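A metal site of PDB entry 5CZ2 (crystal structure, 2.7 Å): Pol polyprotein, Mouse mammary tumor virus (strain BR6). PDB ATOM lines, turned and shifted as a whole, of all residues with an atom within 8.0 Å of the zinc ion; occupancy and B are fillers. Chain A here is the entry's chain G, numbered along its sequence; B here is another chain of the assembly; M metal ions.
The side-chain sulfur of Cys 37 lies close to the backbone NH of Asn 39 (3.6 Å). A ring nitrogen (ND1) of His 9 lies within hydrogen-bond range of the backbone carbonyl oxygen (O) of Gln 14, at 2.9 Å. The backbone carbonyl oxygen of His 13 is in hydrogen-bond range of the side-chain amide nitrogen of Gln 167 of chain B (2.9 Å). A ring nitrogen (NE2) of His 13 sits close to the side-chain amide nitrogen of Asn 39, at 3.3 Å. A ring nitrogen (NE2) of His 13 is in hydrogen-bond range of the backbone carbonyl oxygen (O) of Ala 10 (3.3 Å).
Within 4 Å of the zinc ion: His 9, His 13, Cys 37 and Cys 40.
The zinc ion is bound by ND1 of His 13 (2.0 Å), NE2 of His 9 (2.0 Å), SG of Cys 40 (2.3 Å) and SG of Cys 37 (2.3 Å). The zinc ion has four donor atoms within binding distance.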
ATOM      1  N   GLN A   6      -0.718  22.540  18.999  1.00  0.00           N
ATOM      2  CA  GLN A   6      -0.573  21.890  20.293  1.00  0.00           C
ATOM      3  C   GLN A   6      -1.419  22.563  21.369  1.00  0.00           C
ATOM      4  O   GLN A   6      -2.222  21.912  22.043  1.00  0.00           O
ATOM      5  CB  GLN A   6       0.902  21.864  20.702  1.00  0.00           C
ATOM      6  CG  GLN A   6       1.670  20.676  20.162  1.00  0.00           C
ATOM      7  CD  GLN A   6       3.158  20.779  20.427  1.00  0.00           C
ATOM      8  OE1 GLN A   6       3.727  21.869  20.441  1.00  0.00           O
ATOM      9  NE2 GLN A   6       3.808  19.632  20.650  1.00  0.00           N
ATOM     10  N   SER A   8      -3.863  24.595  21.055  1.00  0.00           N
ATOM     11  CA  SER A   8      -5.295  24.610  20.764  1.00  0.00           C
ATOM     12  C   SER A   8      -5.947  23.312  21.193  1.00  0.00           C
ATOM     13  O   SER A   8      -7.075  23.327  21.725  1.00  0.00           O
ATOM     14  CB  SER A   8      -5.519  24.866  19.273  1.00  0.00           C
ATOM     15  OG  SER A   8      -6.799  25.428  19.053  1.00  0.00           O
ATOM     16  N   HIS A   9      -5.281  22.181  20.972  1.00  0.00           N
ATOM     17  CA  HIS A   9      -5.807  20.913  21.480  1.00  0.00           C
ATOM     18  C   HIS A   9      -5.840  20.900  23.004  1.00  0.00           C
ATOM     19  O   HIS A   9      -6.729  20.273  23.597  1.00  0.00           O
ATOM     20  CB  HIS A   9      -4.969  19.748  20.961  1.00  0.00           C
ATOM     21  CG  HIS A   9      -5.442  18.414  21.445  1.00  0.00           C
ATOM     22  ND1 HIS A   9      -6.345  17.635  20.744  1.00  0.00           N
ATOM     23  CD2 HIS A   9      -5.147  17.715  22.566  1.00  0.00           C
ATOM     24  CE1 HIS A   9      -6.572  16.523  21.402  1.00  0.00           C
ATOM     25  NE2 HIS A   9      -5.867  16.543  22.523  1.00  0.00           N
ATOM     26  N   ALA A  10      -4.898  21.581  23.647  1.00  0.00           N
ATOM     27  CA  ALA A  10      -4.917  21.671  25.107  1.00  0.00           C
ATOM     28  C   ALA A  10      -6.150  22.397  25.619  1.00  0.00           C
ATOM     29  O   ALA A  10      -6.546  22.192  26.764  1.00  0.00           O
ATOM     30  CB  ALA A  10      -3.648  22.370  25.609  1.00  0.00           C
ATOM     31  N   LEU A  11      -6.756  23.249  24.783  1.00  0.00           N
ATOM     32  CA  LEU A  11      -7.959  23.990  25.150  1.00  0.00           C
ATOM     33  C   LEU A  11      -9.227  23.206  24.833  1.00  0.00           C
ATOM     34  O   LEU A  11     -10.103  23.059  25.691  1.00  0.00           O
ATOM     35  CB  LEU A  11      -7.968  25.350  24.437  1.00  0.00           C
ATOM     36  CG  LEU A  11      -9.147  26.281  24.715  1.00  0.00           C
ATOM     37  CD1 LEU A  11      -9.321  26.501  26.208  1.00  0.00           C
ATOM     38  CD2 LEU A  11      -8.946  27.608  23.997  1.00  0.00           C
ATOM     39  N   HIS A  12      -9.349  22.698  23.599  1.00  0.00           N
ATOM     40  CA  HIS A  12     -10.581  22.073  23.143  1.00  0.00           C
ATOM     41  C   HIS A  12     -10.503  20.553  23.064  1.00  0.00           C
ATOM     42  O   HIS A  12     -11.552  19.895  23.116  1.00  0.00           O
ATOM     43  CB  HIS A  12     -10.975  22.607  21.751  1.00  0.00           C
ATOM     44  CG  HIS A  12     -11.027  24.098  21.680  1.00  0.00           C
ATOM     45  ND1 HIS A  12     -12.151  24.824  22.031  1.00  0.00           N
ATOM     46  CD2 HIS A  12     -10.099  25.014  21.298  1.00  0.00           C
ATOM     47  CE1 HIS A  12     -11.908  26.115  21.863  1.00  0.00           C
ATOM     48  NE2 HIS A  12     -10.675  26.249  21.419  1.00  0.00           N
ATOM     49  N   HIS A  13      -9.305  19.976  22.928  1.00  0.00           N
ATOM     50  CA  HIS A  13      -9.121  18.537  22.786  1.00  0.00           C
ATOM     51  C   HIS A  13      -9.903  17.985  21.599  1.00  0.00           C
ATOM     52  O   HIS A  13     -10.579  16.953  21.698  1.00  0.00           O
ATOM     53  CB  HIS A  13      -9.476  17.795  24.081  1.00  0.00           C
ATOM     54  CG  HIS A  13      -8.653  18.223  25.256  1.00  0.00           C
ATOM     55  ND1 HIS A  13      -7.398  17.723  25.509  1.00  0.00           N
ATOM     56  CD2 HIS A  13      -8.904  19.112  26.258  1.00  0.00           C
ATOM     57  CE1 HIS A  13      -6.902  18.280  26.601  1.00  0.00           C
ATOM     58  NE2 HIS A  13      -7.807  19.127  27.074  1.00  0.00           N
ATOM     59  N   GLN A  14      -9.804  18.681  20.479  1.00  0.00           N
ATOM     60  CA  GLN A  14     -10.419  18.221  19.241  1.00  0.00           C
ATOM     61  C   GLN A  14      -9.624  17.056  18.665  1.00  0.00           C
ATOM     62  O   GLN A  14      -8.510  16.743  19.088  1.00  0.00           O
ATOM     63  CB  GLN A  14     -10.502  19.367  18.230  1.00  0.00           C
ATOM     64  CG  GLN A  14      -9.159  19.920  17.776  1.00  0.00           C
ATOM     65  CD  GLN A  14      -8.666  21.056  18.654  1.00  0.00           C
ATOM     66  OE1 GLN A  14      -8.781  21.006  19.877  1.00  0.00           O
ATOM     67  NE2 GLN A  14      -8.129  22.090  18.028  1.00  0.00           N
ATOM     68  N   ASN A  15     -10.205  16.400  17.660  1.00  0.00           N
ATOM     69  CA  ASN A  15      -9.571  15.243  17.057  1.00  0.00           C
ATOM     70  C   ASN A  15      -8.412  15.665  16.157  1.00  0.00           C
ATOM     71  O   ASN A  15      -8.169  16.854  15.921  1.00  0.00           O
ATOM     72  CB  ASN A  15     -10.599  14.421  16.271  1.00  0.00           C
ATOM     73  CG  ASN A  15     -11.356  15.237  15.238  1.00  0.00           C
ATOM     74  OD1 ASN A  15     -10.982  16.369  14.940  1.00  0.00           O
ATOM     75  ND2 ASN A  15     -12.411  14.662  14.685  1.00  0.00           N
ATOM     76  N   LEU A  19      -7.082  19.275  13.982  1.00  0.00           N
ATOM     77  CA  LEU A  19      -5.740  19.844  14.098  1.00  0.00           C
ATOM     78  C   LEU A  19      -5.012  19.832  12.772  1.00  0.00           C
ATOM     79  O   LEU A  19      -4.201  20.734  12.509  1.00  0.00           O
ATOM     80  CB  LEU A  19      -4.942  19.068  15.149  1.00  0.00           C
ATOM     81  CG  LEU A  19      -5.451  19.112  16.591  1.00  0.00           C
ATOM     82  CD1 LEU A  19      -4.669  18.128  17.458  1.00  0.00           C
ATOM     83  CD2 LEU A  19      -5.346  20.513  17.149  1.00  0.00           C
ATOM     84  N   ILE A  33      -0.206  14.307  18.707  1.00  0.00           N
ATOM     85  CA  ILE A  33      -0.677  15.244  19.715  1.00  0.00           C
ATOM     86  C   ILE A  33      -1.774  14.604  20.572  1.00  0.00           C
ATOM     87  O   ILE A  33      -1.833  14.798  21.781  1.00  0.00           O
ATOM     88  CB  ILE A  33      -1.160  16.550  19.062  1.00  0.00           C
ATOM     89  CG1 ILE A  33       0.025  17.320  18.466  1.00  0.00           C
ATOM     90  CG2 ILE A  33      -1.901  17.419  20.058  1.00  0.00           C
ATOM     91  CD1 ILE A  33      -0.368  18.591  17.752  1.00  0.00           C
ATOM     92  N   VAL A  34      -2.657  13.822  19.934  1.00  0.00           N
ATOM     93  CA  VAL A  34      -3.767  13.223  20.656  1.00  0.00           C
ATOM     94  C   VAL A  34      -3.273  12.150  21.616  1.00  0.00           C
ATOM     95  O   VAL A  34      -3.709  12.078  22.769  1.00  0.00           O
ATOM     96  CB  VAL A  34      -4.809  12.668  19.667  1.00  0.00           C
ATOM     97  CG1 VAL A  34      -5.947  11.997  20.413  1.00  0.00           C
ATOM     98  CG2 VAL A  34      -5.341  13.788  18.777  1.00  0.00           C
ATOM     99  N   LYS A  35      -2.361  11.292  21.150  1.00  0.00           N
ATOM    100  CA  LYS A  35      -1.745  10.314  22.035  1.00  0.00           C
ATOM    101  C   LYS A  35      -0.962  10.991  23.144  1.00  0.00           C
ATOM    102  O   LYS A  35      -1.110  10.659  24.325  1.00  0.00           O
ATOM    103  CB  LYS A  35      -0.843   9.376  21.229  1.00  0.00           C
ATOM    104  CG  LYS A  35      -1.568   8.602  20.134  1.00  0.00           C
ATOM    105  CD  LYS A  35      -2.717   7.790  20.702  1.00  0.00           C
ATOM    106  CE  LYS A  35      -3.458   7.041  19.603  1.00  0.00           C
ATOM    107  NZ  LYS A  35      -4.621   6.287  20.141  1.00  0.00           N
ATOM    108  N   LEU A  36      -0.120  11.971  22.787  1.00  0.00           N
ATOM    109  CA  LEU A  36       0.656  12.704  23.778  1.00  0.00           C
ATOM    110  C   LEU A  36      -0.223  13.461  24.762  1.00  0.00           C
ATOM    111  O   LEU A  36       0.223  13.764  25.875  1.00  0.00           O
ATOM    112  CB  LEU A  36       1.626  13.663  23.071  1.00  0.00           C
ATOM    113  CG  LEU A  36       2.697  14.360  23.902  1.00  0.00           C
ATOM    114  CD1 LEU A  36       3.682  13.347  24.477  1.00  0.00           C
ATOM    115  CD2 LEU A  36       3.421  15.403  23.076  1.00  0.00           C
ATOM    116  N   CYS A  37      -1.455  13.786  24.379  1.00  0.00           N
ATOM    117  CA  CYS A  37      -2.349  14.488  25.293  1.00  0.00           C
ATOM    118  C   CYS A  37      -2.811  13.544  26.387  1.00  0.00           C
ATOM    119  O   CYS A  37      -3.346  12.472  26.092  1.00  0.00           O
ATOM    120  CB  CYS A  37      -3.551  15.060  24.536  1.00  0.00           C
ATOM    121  SG  CYS A  37      -4.756  15.911  25.578  1.00  0.00           S
ATOM    122  N   PRO A  38      -2.648  13.905  27.665  1.00  0.00           N
ATOM    123  CA  PRO A  38      -3.037  12.992  28.743  1.00  0.00           C
ATOM    124  C   PRO A  38      -4.535  12.811  28.884  1.00  0.00           C
ATOM    125  O   PRO A  38      -4.971  11.844  29.521  1.00  0.00           O
ATOM    126  CB  PRO A  38      -2.436  13.637  29.996  1.00  0.00           C
ATOM    127  CG  PRO A  38      -1.422  14.637  29.487  1.00  0.00           C
ATOM    128  CD  PRO A  38      -1.957  15.105  28.174  1.00  0.00           C
ATOM    129  N   ASN A  39      -5.346  13.720  28.325  1.00  0.00           N
ATOM    130  CA  ASN A  39      -6.792  13.654  28.452  1.00  0.00           C
ATOM    131  C   ASN A  39      -7.457  12.916  27.291  1.00  0.00           C
ATOM    132  O   ASN A  39      -8.687  12.877  27.230  1.00  0.00           O
ATOM    133  CB  ASN A  39      -7.363  15.070  28.562  1.00  0.00           C
ATOM    134  CG  ASN A  39      -6.652  15.914  29.598  1.00  0.00           C
ATOM    135  OD1 ASN A  39      -5.919  15.393  30.436  1.00  0.00           O
ATOM    136  ND2 ASN A  39      -6.844  17.220  29.525  1.00  0.00           N
ATOM    137  N   CYS A  40      -6.680  12.337  26.391  1.00  0.00           N
ATOM    138  CA  CYS A  40      -7.195  11.754  25.158  1.00  0.00           C
ATOM    139  C   CYS A  40      -6.619  10.353  24.975  1.00  0.00           C
ATOM    140  O   CYS A  40      -5.585  10.183  24.316  1.00  0.00           O
ATOM    141  CB  CYS A  40      -6.882  12.637  23.947  1.00  0.00           C
ATOM    142  SG  CYS A  40      -7.757  14.223  23.950  1.00  0.00           S
ATOM    143  N   PRO A  41      -7.257   9.328  25.557  1.00  0.00           N
ATOM    144  CA  PRO A  41      -6.785   7.945  25.439  1.00  0.00           C
ATOM    145  C   PRO A  41      -7.372   7.242  24.216  1.00  0.00           C
ATOM    146  O   PRO A  41      -7.365   7.822  23.133  1.00  0.00           O
ATOM    147  CB  PRO A  41      -7.279   7.306  26.738  1.00  0.00           C
ATOM    148  CG  PRO A  41      -8.453   8.171  27.194  1.00  0.00           C
ATOM    149  CD  PRO A  41      -8.504   9.413  26.341  1.00  0.00           C
ATOM    150  N   GLN B 167     -16.166  13.836  25.428  1.00  0.00           N
ATOM    151  CA  GLN B 167     -15.697  15.210  25.343  1.00  0.00           C
ATOM    152  C   GLN B 167     -15.828  15.932  26.681  1.00  0.00           C
ATOM    153  O   GLN B 167     -14.975  16.751  27.045  1.00  0.00           O
ATOM    154  CB  GLN B 167     -16.454  15.964  24.259  1.00  0.00           C
ATOM    155  CG  GLN B 167     -15.713  16.071  22.939  1.00  0.00           C
ATOM    156  CD  GLN B 167     -14.459  16.933  23.047  1.00  0.00           C
ATOM    157  OE1 GLN B 167     -14.472  17.992  23.667  1.00  0.00           O
ATOM    158  NE2 GLN B 167     -13.371  16.469  22.432  1.00  0.00           N
ATOM    159  N   LYS B 170     -12.828  15.174  28.928  1.00  0.00           N
ATOM    160  CA  LYS B 170     -11.584  15.822  28.517  1.00  0.00           C
ATOM    161  C   LYS B 170     -11.532  17.285  28.941  1.00  0.00           C
ATOM    162  O   LYS B 170     -10.437  17.818  29.174  1.00  0.00           O
ATOM    163  CB  LYS B 170     -11.430  15.720  26.999  1.00  0.00           C
ATOM    164  CG  LYS B 170     -11.579  14.309  26.444  1.00  0.00           C
ATOM    165  CD  LYS B 170     -11.187  14.261  24.970  1.00  0.00           C
ATOM    166  CE  LYS B 170     -12.092  13.332  24.189  1.00  0.00           C
ATOM    167  NZ  LYS B 170     -11.497  12.923  22.888  1.00  0.00           N
ATOM    168  N   LEU B 171     -12.681  17.940  29.057  1.00  0.00           N
ATOM    169  CA  LEU B 171     -12.706  19.397  29.236  1.00  0.00           C
ATOM    170  C   LEU B 171     -12.452  19.828  30.677  1.00  0.00           C
ATOM    171  O   LEU B 171     -12.027  20.973  30.886  1.00  0.00           O
ATOM    172  CB  LEU B 171     -14.048  19.957  28.761  1.00  0.00           C
ATOM    173  CG  LEU B 171     -14.251  19.965  27.240  1.00  0.00           C
ATOM    174  CD1 LEU B 171     -15.546  20.674  26.871  1.00  0.00           C
ATOM    175  CD2 LEU B 171     -13.058  20.609  26.545  1.00  0.00           C
HETATM  176 ZN    ZN M   1      -6.713  16.224  24.349  1.00  0.00          ZN
